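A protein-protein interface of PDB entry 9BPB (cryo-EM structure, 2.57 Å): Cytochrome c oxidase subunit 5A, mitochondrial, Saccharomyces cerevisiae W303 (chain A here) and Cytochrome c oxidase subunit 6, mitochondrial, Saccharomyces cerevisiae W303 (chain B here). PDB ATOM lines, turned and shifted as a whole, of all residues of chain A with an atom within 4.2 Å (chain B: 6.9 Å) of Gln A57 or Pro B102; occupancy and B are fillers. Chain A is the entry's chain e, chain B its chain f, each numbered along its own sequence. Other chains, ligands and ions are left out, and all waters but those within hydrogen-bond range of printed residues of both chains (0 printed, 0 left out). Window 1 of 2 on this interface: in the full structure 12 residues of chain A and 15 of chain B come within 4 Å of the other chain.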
ATOM      1  N   LEU A  53       2.722  26.908 -21.847  1.00  0.00           N
ATOM      2  CA  LEU A  53       3.324  26.177 -20.737  1.00  0.00           C
ATOM      3  C   LEU A  53       4.529  25.365 -21.192  1.00  0.00           C
ATOM      4  O   LEU A  53       5.517  25.243 -20.459  1.00  0.00           O
ATOM      5  CB  LEU A  53       2.280  25.269 -20.085  1.00  0.00           C
ATOM      6  CG  LEU A  53       1.284  25.935 -19.134  1.00  0.00           C
ATOM      7  CD1 LEU A  53       0.416  24.897 -18.439  1.00  0.00           C
ATOM      8  CD2 LEU A  53       2.009  26.796 -18.113  1.00  0.00           C
ATOM      9  N   SER A  54       4.467  24.801 -22.400  1.00  0.00           N
ATOM     10  CA  SER A  54       5.554  23.956 -22.882  1.00  0.00           C
ATOM     11  C   SER A  54       6.827  24.761 -23.122  1.00  0.00           C
ATOM     12  O   SER A  54       7.929  24.299 -22.805  1.00  0.00           O
ATOM     13  CB  SER A  54       5.128  23.232 -24.157  1.00  0.00           C
ATOM     14  OG  SER A  54       4.099  22.300 -23.891  1.00  0.00           O
ATOM     15  N   GLU A  55       6.697  25.961 -23.690  1.00  0.00           N
ATOM     16  CA  GLU A  55       7.877  26.769 -23.989  1.00  0.00           C
ATOM     17  C   GLU A  55       8.571  27.243 -22.718  1.00  0.00           C
ATOM     18  O   GLU A  55       9.805  27.284 -22.657  1.00  0.00           O
ATOM     19  CB  GLU A  55       7.494  27.962 -24.863  1.00  0.00           C
ATOM     20  CG  GLU A  55       7.155  27.596 -26.292  1.00  0.00           C
ATOM     21  CD  GLU A  55       8.361  27.084 -27.054  1.00  0.00           C
ATOM     22  OE1 GLU A  55       9.488  27.521 -26.747  1.00  0.00           O
ATOM     23  OE2 GLU A  55       8.182  26.244 -27.963  1.00  0.00           O
ATOM     24  N   ARG A  56       7.799  27.612 -21.699  1.00  0.00           N
ATOM     25  CA  ARG A  56       8.393  28.137 -20.478  1.00  0.00           C
ATOM     26  C   ARG A  56       9.076  27.050 -19.657  1.00  0.00           C
ATOM     27  O   ARG A  56       9.913  27.367 -18.805  1.00  0.00           O
ATOM     28  CB  ARG A  56       7.319  28.853 -19.655  1.00  0.00           C
ATOM     29  CG  ARG A  56       7.846  29.638 -18.470  1.00  0.00           C
ATOM     30  CD  ARG A  56       6.817  30.632 -17.967  1.00  0.00           C
ATOM     31  NE  ARG A  56       7.132  31.099 -16.624  1.00  0.00           N
ATOM     32  CZ  ARG A  56       8.055  32.009 -16.344  1.00  0.00           C
ATOM     33  NH1 ARG A  56       8.771  32.584 -17.296  1.00  0.00           N
ATOM     34  NH2 ARG A  56       8.265  32.350 -15.076  1.00  0.00           N
ATOM     35  N   GLN A  57       8.757  25.776 -19.906  1.00  0.00           N
ATOM     36  CA  GLN A  57       9.457  24.694 -19.220  1.00  0.00           C
ATOM     37  C   GLN A  57      10.853  24.477 -19.788  1.00  0.00           C
ATOM     38  O   GLN A  57      11.757  24.060 -19.055  1.00  0.00           O
ATOM     39  CB  GLN A  57       8.657  23.396 -19.301  1.00  0.00           C
ATOM     40  CG  GLN A  57       7.364  23.400 -18.510  1.00  0.00           C
ATOM     41  CD  GLN A  57       6.769  22.015 -18.379  1.00  0.00           C
ATOM     42  OE1 GLN A  57       7.383  21.026 -18.772  1.00  0.00           O
ATOM     43  NE2 GLN A  57       5.567  21.937 -17.830  1.00  0.00           N
ATOM     44  N   LYS A  58      11.055  24.756 -21.076  1.00  0.00           N
ATOM     45  CA  LYS A  58      12.369  24.616 -21.705  1.00  0.00           C
ATOM     46  C   LYS A  58      13.248  25.811 -21.334  1.00  0.00           C
ATOM     47  O   LYS A  58      13.784  26.532 -22.175  1.00  0.00           O
ATOM     48  CB  LYS A  58      12.223  24.479 -23.215  1.00  0.00           C
ATOM     49  CG  LYS A  58      11.433  23.262 -23.658  1.00  0.00           C
ATOM     50  CD  LYS A  58      11.642  22.979 -25.134  1.00  0.00           C
ATOM     51  CE  LYS A  58      10.991  24.041 -26.000  1.00  0.00           C
ATOM     52  NZ  LYS A  58      11.114  23.718 -27.447  1.00  0.00           N
ATOM     53  N   LEU A  59      13.390  26.000 -20.023  1.00  0.00           N
ATOM     54  CA  LEU A  59      14.033  27.148 -19.410  1.00  0.00           C
ATOM     55  C   LEU A  59      14.392  26.709 -18.004  1.00  0.00           C
ATOM     56  O   LEU A  59      13.634  25.926 -17.415  1.00  0.00           O
ATOM     57  CB  LEU A  59      13.089  28.356 -19.387  1.00  0.00           C
ATOM     58  CG  LEU A  59      13.608  29.747 -19.035  1.00  0.00           C
ATOM     59  CD1 LEU A  59      14.509  30.267 -20.141  1.00  0.00           C
ATOM     60  CD2 LEU A  59      12.453  30.698 -18.795  1.00  0.00           C
ATOM     61  N   TRP A  61      14.438  25.861 -14.374  1.00  0.00           N
ATOM     62  CA  TRP A  61      13.418  25.969 -13.346  1.00  0.00           C
ATOM     63  C   TRP A  61      13.975  26.734 -12.147  1.00  0.00           C
ATOM     64  O   TRP A  61      15.120  27.195 -12.148  1.00  0.00           O
ATOM     65  CB  TRP A  61      12.903  24.584 -12.960  1.00  0.00           C
ATOM     66  CG  TRP A  61      12.583  23.714 -14.147  1.00  0.00           C
ATOM     67  CD1 TRP A  61      12.125  24.129 -15.364  1.00  0.00           C
ATOM     68  CD2 TRP A  61      12.700  22.288 -14.229  1.00  0.00           C
ATOM     69  NE1 TRP A  61      11.951  23.053 -16.197  1.00  0.00           N
ATOM     70  CE2 TRP A  61      12.297  21.911 -15.525  1.00  0.00           C
ATOM     71  CE3 TRP A  61      13.108  21.295 -13.333  1.00  0.00           C
ATOM     72  CZ2 TRP A  61      12.289  20.583 -15.947  1.00  0.00           C
ATOM     73  CZ3 TRP A  61      13.097  19.977 -13.755  1.00  0.00           C
ATOM     74  CH2 TRP A  61      12.691  19.634 -15.050  1.00  0.00           C
ATOM     75  N   VAL A  72       0.874  23.111 -14.374  1.00  0.00           N
ATOM     76  CA  VAL A  72       1.426  22.047 -15.203  1.00  0.00           C
ATOM     77  C   VAL A  72       1.213  20.690 -14.546  1.00  0.00           C
ATOM     78  O   VAL A  72       0.994  19.685 -15.228  1.00  0.00           O
ATOM     79  CB  VAL A  72       2.915  22.311 -15.503  1.00  0.00           C
ATOM     80  CG1 VAL A  72       3.075  23.589 -16.307  1.00  0.00           C
ATOM     81  CG2 VAL A  72       3.726  22.386 -14.220  1.00  0.00           C
ATOM     82  N   SER A  76      -1.072  17.485 -16.200  1.00  0.00           N
ATOM     83  CA  SER A  76      -0.443  16.179 -16.347  1.00  0.00           C
ATOM     84  C   SER A  76      -1.121  15.124 -15.480  1.00  0.00           C
ATOM     85  O   SER A  76      -1.433  14.027 -15.956  1.00  0.00           O
ATOM     86  CB  SER A  76       1.043  16.273 -16.012  1.00  0.00           C
ATOM     87  OG  SER A  76       1.768  16.843 -17.084  1.00  0.00           O
ATOM     88  N   TYR A  77      -1.366  15.436 -14.203  1.00  0.00           N
ATOM     89  CA  TYR A  77      -1.744  14.409 -13.238  1.00  0.00           C
ATOM     90  C   TYR A  77      -3.041  14.724 -12.498  1.00  0.00           C
ATOM     91  O   TYR A  77      -3.273  14.175 -11.418  1.00  0.00           O
ATOM     92  CB  TYR A  77      -0.612  14.184 -12.232  1.00  0.00           C
ATOM     93  CG  TYR A  77       0.665  13.687 -12.866  1.00  0.00           C
ATOM     94  CD1 TYR A  77       0.738  12.418 -13.423  1.00  0.00           C
ATOM     95  CD2 TYR A  77       1.795  14.489 -12.913  1.00  0.00           C
ATOM     96  CE1 TYR A  77       1.897  11.962 -14.006  1.00  0.00           C
ATOM     97  CE2 TYR A  77       2.962  14.040 -13.493  1.00  0.00           C
ATOM     98  CZ  TYR A  77       3.008  12.776 -14.038  1.00  0.00           C
ATOM     99  OH  TYR A  77       4.170  12.328 -14.618  1.00  0.00           O
ATOM    100  N   LEU B  66       9.927  12.242 -24.281  1.00  0.00           N
ATOM    101  CA  LEU B  66       9.154  12.258 -23.046  1.00  0.00           C
ATOM    102  C   LEU B  66       8.300  11.004 -22.898  1.00  0.00           C
ATOM    103  O   LEU B  66       7.847  10.705 -21.790  1.00  0.00           O
ATOM    104  CB  LEU B  66       8.299  13.529 -23.015  1.00  0.00           C
ATOM    105  CG  LEU B  66       7.620  14.033 -21.740  1.00  0.00           C
ATOM    106  CD1 LEU B  66       7.488  15.541 -21.834  1.00  0.00           C
ATOM    107  CD2 LEU B  66       6.262  13.417 -21.542  1.00  0.00           C
ATOM    108  N   ARG B  96      15.007  16.664 -16.739  1.00  0.00           N
ATOM    109  CA  ARG B  96      15.596  17.920 -17.190  1.00  0.00           C
ATOM    110  C   ARG B  96      16.009  17.852 -18.656  1.00  0.00           C
ATOM    111  O   ARG B  96      15.949  18.864 -19.364  1.00  0.00           O
ATOM    112  CB  ARG B  96      16.793  18.268 -16.304  1.00  0.00           C
ATOM    113  CG  ARG B  96      17.701  19.378 -16.824  1.00  0.00           C
ATOM    114  CD  ARG B  96      17.119  20.764 -16.591  1.00  0.00           C
ATOM    115  NE  ARG B  96      16.333  21.234 -17.724  1.00  0.00           N
ATOM    116  CZ  ARG B  96      15.669  22.381 -17.748  1.00  0.00           C
ATOM    117  NH1 ARG B  96      15.670  23.201 -16.711  1.00  0.00           N
ATOM    118  NH2 ARG B  96      14.992  22.717 -18.841  1.00  0.00           N
ATOM    119  N   VAL B  98      14.536  16.064 -21.130  1.00  0.00           N
ATOM    120  CA  VAL B  98      13.362  16.135 -21.996  1.00  0.00           C
ATOM    121  C   VAL B  98      12.438  17.292 -21.639  1.00  0.00           C
ATOM    122  O   VAL B  98      11.368  17.424 -22.247  1.00  0.00           O
ATOM    123  CB  VAL B  98      12.560  14.816 -21.977  1.00  0.00           C
ATOM    124  CG1 VAL B  98      13.424  13.663 -22.453  1.00  0.00           C
ATOM    125  CG2 VAL B  98      12.003  14.546 -20.593  1.00  0.00           C
ATOM    126  N   ASN B  99      12.814  18.127 -20.667  1.00  0.00           N
ATOM    127  CA  ASN B  99      12.099  19.361 -20.337  1.00  0.00           C
ATOM    128  C   ASN B  99      10.653  19.082 -19.910  1.00  0.00           C
ATOM    129  O   ASN B  99       9.694  19.529 -20.539  1.00  0.00           O
ATOM    130  CB  ASN B  99      12.138  20.342 -21.512  1.00  0.00           C
ATOM    131  CG  ASN B  99      13.537  20.550 -22.052  1.00  0.00           C
ATOM    132  OD1 ASN B  99      14.436  20.982 -21.332  1.00  0.00           O
ATOM    133  ND2 ASN B  99      13.728  20.245 -23.330  1.00  0.00           N
ATOM    134  N   ASP B 100      10.511  18.331 -18.816  1.00  0.00           N
ATOM    135  CA  ASP B 100       9.195  18.053 -18.238  1.00  0.00           C
ATOM    136  C   ASP B 100       9.298  18.207 -16.724  1.00  0.00           C
ATOM    137  O   ASP B 100       9.797  17.313 -16.034  1.00  0.00           O
ATOM    138  CB  ASP B 100       8.696  16.662 -18.617  1.00  0.00           C
ATOM    139  CG  ASP B 100       7.299  16.380 -18.090  1.00  0.00           C
ATOM    140  OD1 ASP B 100       7.145  16.193 -16.867  1.00  0.00           O
ATOM    141  OD2 ASP B 100       6.349  16.347 -18.898  1.00  0.00           O
ATOM    142  N   LEU B 101       8.827  19.342 -16.216  1.00  0.00           N
ATOM    143  CA  LEU B 101       8.786  19.555 -14.769  1.00  0.00           C
ATOM    144  C   LEU B 101       7.858  18.587 -14.039  1.00  0.00           C
ATOM    145  O   LEU B 101       8.272  18.044 -13.000  1.00  0.00           O
ATOM    146  CB  LEU B 101       8.413  21.012 -14.480  1.00  0.00           C
ATOM    147  CG  LEU B 101       8.386  21.456 -13.017  1.00  0.00           C
ATOM    148  CD1 LEU B 101       9.725  21.207 -12.343  1.00  0.00           C
ATOM    149  CD2 LEU B 101       8.006  22.921 -12.923  1.00  0.00           C
ATOM    150  N   PRO B 102       6.619  18.334 -14.485  1.00  0.00           N
ATOM    151  CA  PRO B 102       5.716  17.503 -13.670  1.00  0.00           C
ATOM    152  C   PRO B 102       6.168  16.063 -13.472  1.00  0.00           C
ATOM    153  O   PRO B 102       5.742  15.435 -12.496  1.00  0.00           O
ATOM    154  CB  PRO B 102       4.389  17.570 -14.441  1.00  0.00           C
ATOM    155  CG  PRO B 102       4.756  17.990 -15.809  1.00  0.00           C
ATOM    156  CD  PRO B 102       5.910  18.907 -15.642  1.00  0.00           C
ATOM    157  N   THR B 103       6.995  15.503 -14.358  1.00  0.00           N
ATOM    158  CA  THR B 103       7.460  14.139 -14.116  1.00  0.00           C
ATOM    159  C   THR B 103       8.545  14.102 -13.047  1.00  0.00           C
ATOM    160  O   THR B 103       8.662  13.111 -12.321  1.00  0.00           O
ATOM    161  CB  THR B 103       7.951  13.488 -15.414  1.00  0.00           C
ATOM    162  OG1 THR B 103       8.177  12.090 -15.192  1.00  0.00           O
ATOM    163  CG2 THR B 103       9.241  14.118 -15.896  1.00  0.00           C
ATOM    164  N   ALA B 104       9.334  15.171 -12.927  1.00  0.00           N
ATOM    165  CA  ALA B 104      10.314  15.252 -11.852  1.00  0.00           C
ATOM    166  C   ALA B 104       9.630  15.364 -10.496  1.00  0.00           C
ATOM    167  O   ALA B 104      10.114  14.813  -9.501  1.00  0.00           O
ATOM    168  CB  ALA B 104      11.253  16.433 -12.083  1.00  0.00           C
ATOM    169  N   ILE B 105       8.506  16.082 -10.435  1.00  0.00           N
ATOM    170  CA  ILE B 105       7.750  16.177  -9.191  1.00  0.00           C
ATOM    171  C   ILE B 105       7.199  14.814  -8.796  1.00  0.00           C
ATOM    172  O   ILE B 105       7.200  14.446  -7.616  1.00  0.00           O
ATOM    173  CB  ILE B 105       6.631  17.225  -9.326  1.00  0.00           C
ATOM    174  CG1 ILE B 105       7.175  18.510  -9.949  1.00  0.00           C
ATOM    175  CG2 ILE B 105       6.006  17.516  -7.976  1.00  0.00           C
ATOM    176  CD1 ILE B 105       6.111  19.539 -10.245  1.00  0.00           C
ATOM    177  N   ARG B 106       6.726  14.040  -9.774  1.00  0.00           N
ATOM    178  CA  ARG B 106       6.166  12.722  -9.504  1.00  0.00           C
ATOM    179  C   ARG B 106       7.223  11.695  -9.119  1.00  0.00           C
ATOM    180  O   ARG B 106       6.863  10.598  -8.678  1.00  0.00           O
ATOM    181  CB  ARG B 106       5.382  12.235 -10.727  1.00  0.00           C
ATOM    182  CG  ARG B 106       4.435  11.072 -10.461  1.00  0.00           C
ATOM    183  CD  ARG B 106       3.109  11.548  -9.900  1.00  0.00           C
ATOM    184  NE  ARG B 106       2.017  10.638 -10.222  1.00  0.00           N
ATOM    185  CZ  ARG B 106       0.760  10.815  -9.840  1.00  0.00           C
ATOM    186  NH1 ARG B 106       0.401  11.858  -9.111  1.00  0.00           N
ATOM    187  NH2 ARG B 106      -0.159   9.927 -10.199  1.00  0.00           N
ATOM    188  N   VAL B 107       8.510  12.016  -9.272  1.00  0.00           N
ATOM    189  CA  VAL B 107       9.558  11.073  -8.887  1.00  0.00           C
ATOM    190  C   VAL B 107       9.520  10.822  -7.386  1.00  0.00           C
ATOM    191  O   VAL B 107       9.513   9.674  -6.931  1.00  0.00           O
ATOM    192  CB  VAL B 107      10.938  11.586  -9.334  1.00  0.00           C
ATOM    193  CG1 VAL B 107      12.033  10.801  -8.643  1.00  0.00           C
ATOM    194  CG2 VAL B 107      11.082  11.486 -10.840  1.00  0.00           C
ATOM    195  N   GLU B 109       6.985  11.685  -5.415  1.00  0.00           N
ATOM    196  CA  GLU B 109       5.653  11.167  -5.126  1.00  0.00           C
ATOM    197  C   GLU B 109       5.604   9.661  -5.330  1.00  0.00           C
ATOM    198  O   GLU B 109       4.966   8.939  -4.554  1.00  0.00           O
ATOM    199  CB  GLU B 109       4.610  11.850  -6.009  1.00  0.00           C
ATOM    200  CG  GLU B 109       4.668  13.361  -6.007  1.00  0.00           C
ATOM    201  CD  GLU B 109       3.552  13.978  -6.824  1.00  0.00           C
ATOM    202  OE1 GLU B 109       2.629  13.237  -7.218  1.00  0.00           O
ATOM    203  OE2 GLU B 109       3.604  15.197  -7.086  1.00  0.00           O
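Of the 11 printed residues of chain A, 6 touch a printed residue of chain B. Printed residues of chain A that touch a printed residue of chain B: Gln A57, Lys A58, Leu A59, Trp A61, Ser A76 and Tyr A77. Hydrophobic or aromatic side chains of chain A that line the printed part of chain B: Trp A61 and Tyr A77. Among the printed residues, 14 pairs touch across the chains. Among the printed residues, no Asp or Glu carboxylate lies within 4 Å of a Lys or Arg side-chain nitrogen of the other chain.
Pro B102 touches three residues of chain A. Of the printed residues of chain A, Asn B99 touches Gln A57 and Lys A58. Printed residues of chain B within 4 Å of Lys A58: Asn B99 (3.7 Å). Of the printed residues of chain A, Arg B106 touches Tyr A77. Printed residues of chain B within 4 Å of Leu A59: Arg B96 (3.5 Å). Of the printed residues of chain B, Tyr A77 touches Pro B102 (3.3 Å), Thr B103 (3.8 Å) and Arg B106 (3.9 Å). Leu A53 touches none of the printed residues of chain B. The nearest residue of chain B that does not touch Gln A57 is Leu B66 (6.3 Å). The nearest residue of chain A that does not touch Pro B102 is Val A72 (4.1 Å). The nearest printed residue of chain B that does not touch Trp A61 is Ala B104 (4.3 Å).
The guanidinium group (NH1) of Arg B96 lies within hydrogen-bond range of the backbone carbonyl oxygen (O) of Leu A59 (3.5 Å). OE1 of Gln A57 sits close to O of Asn B99, 3.3 Å away. OE1 of Gln A57 is in hydrogen-bond range of N of Leu B101.
OE2 of Glu A55 lies within salt-bridge range of NZ of Lys A58 (3.9 Å). The side-chain carboxylate (OD1) of Asp B100 lies within hydrogen-bond range of the backbone NH (N) of Thr B103, at 2.6 Å. The side-chain carboxylate of Glu B109 is in salt-bridge range of the guanidinium group of Arg B106, 3.2 Å away. The backbone carbonyl oxygen (O) of Val A72 sits at hydrogen-bond distance from the side-chain hydroxyl (OG) of Ser A76 (3.5 Å). O of Gln A57 is in hydrogen-bond range of NE1 of Trp A61, 3.0 Å away. NH2 of Arg B96 is in hydrogen-bond range of OD1 of Asn B99 (3.1 Å).
Arg B96 touches Gln A57. CA of Asp B100 touches OE1 of Gln A57 (3.5 Å). Pro B102 touches Gln A57 (CD to NE2, 3.8 Å). Lys A58 touches Asn B99 (CG to CB, 3.7 Å). O of Asp B100 touches CH2 of Trp A61, 3.8 Å away. Leu B101 touches Trp A61 (CD1 to CE3, 3.5 Å). Pro B102 touches Ser A76. CE2 of Tyr A77 touches O of Pro B102 (3.3 Å). Thr B103 touches Tyr A77 (CA to OH, 3.8 Å). CD1 of Tyr A77 touches NE of Arg B106, at 3.9 Å.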
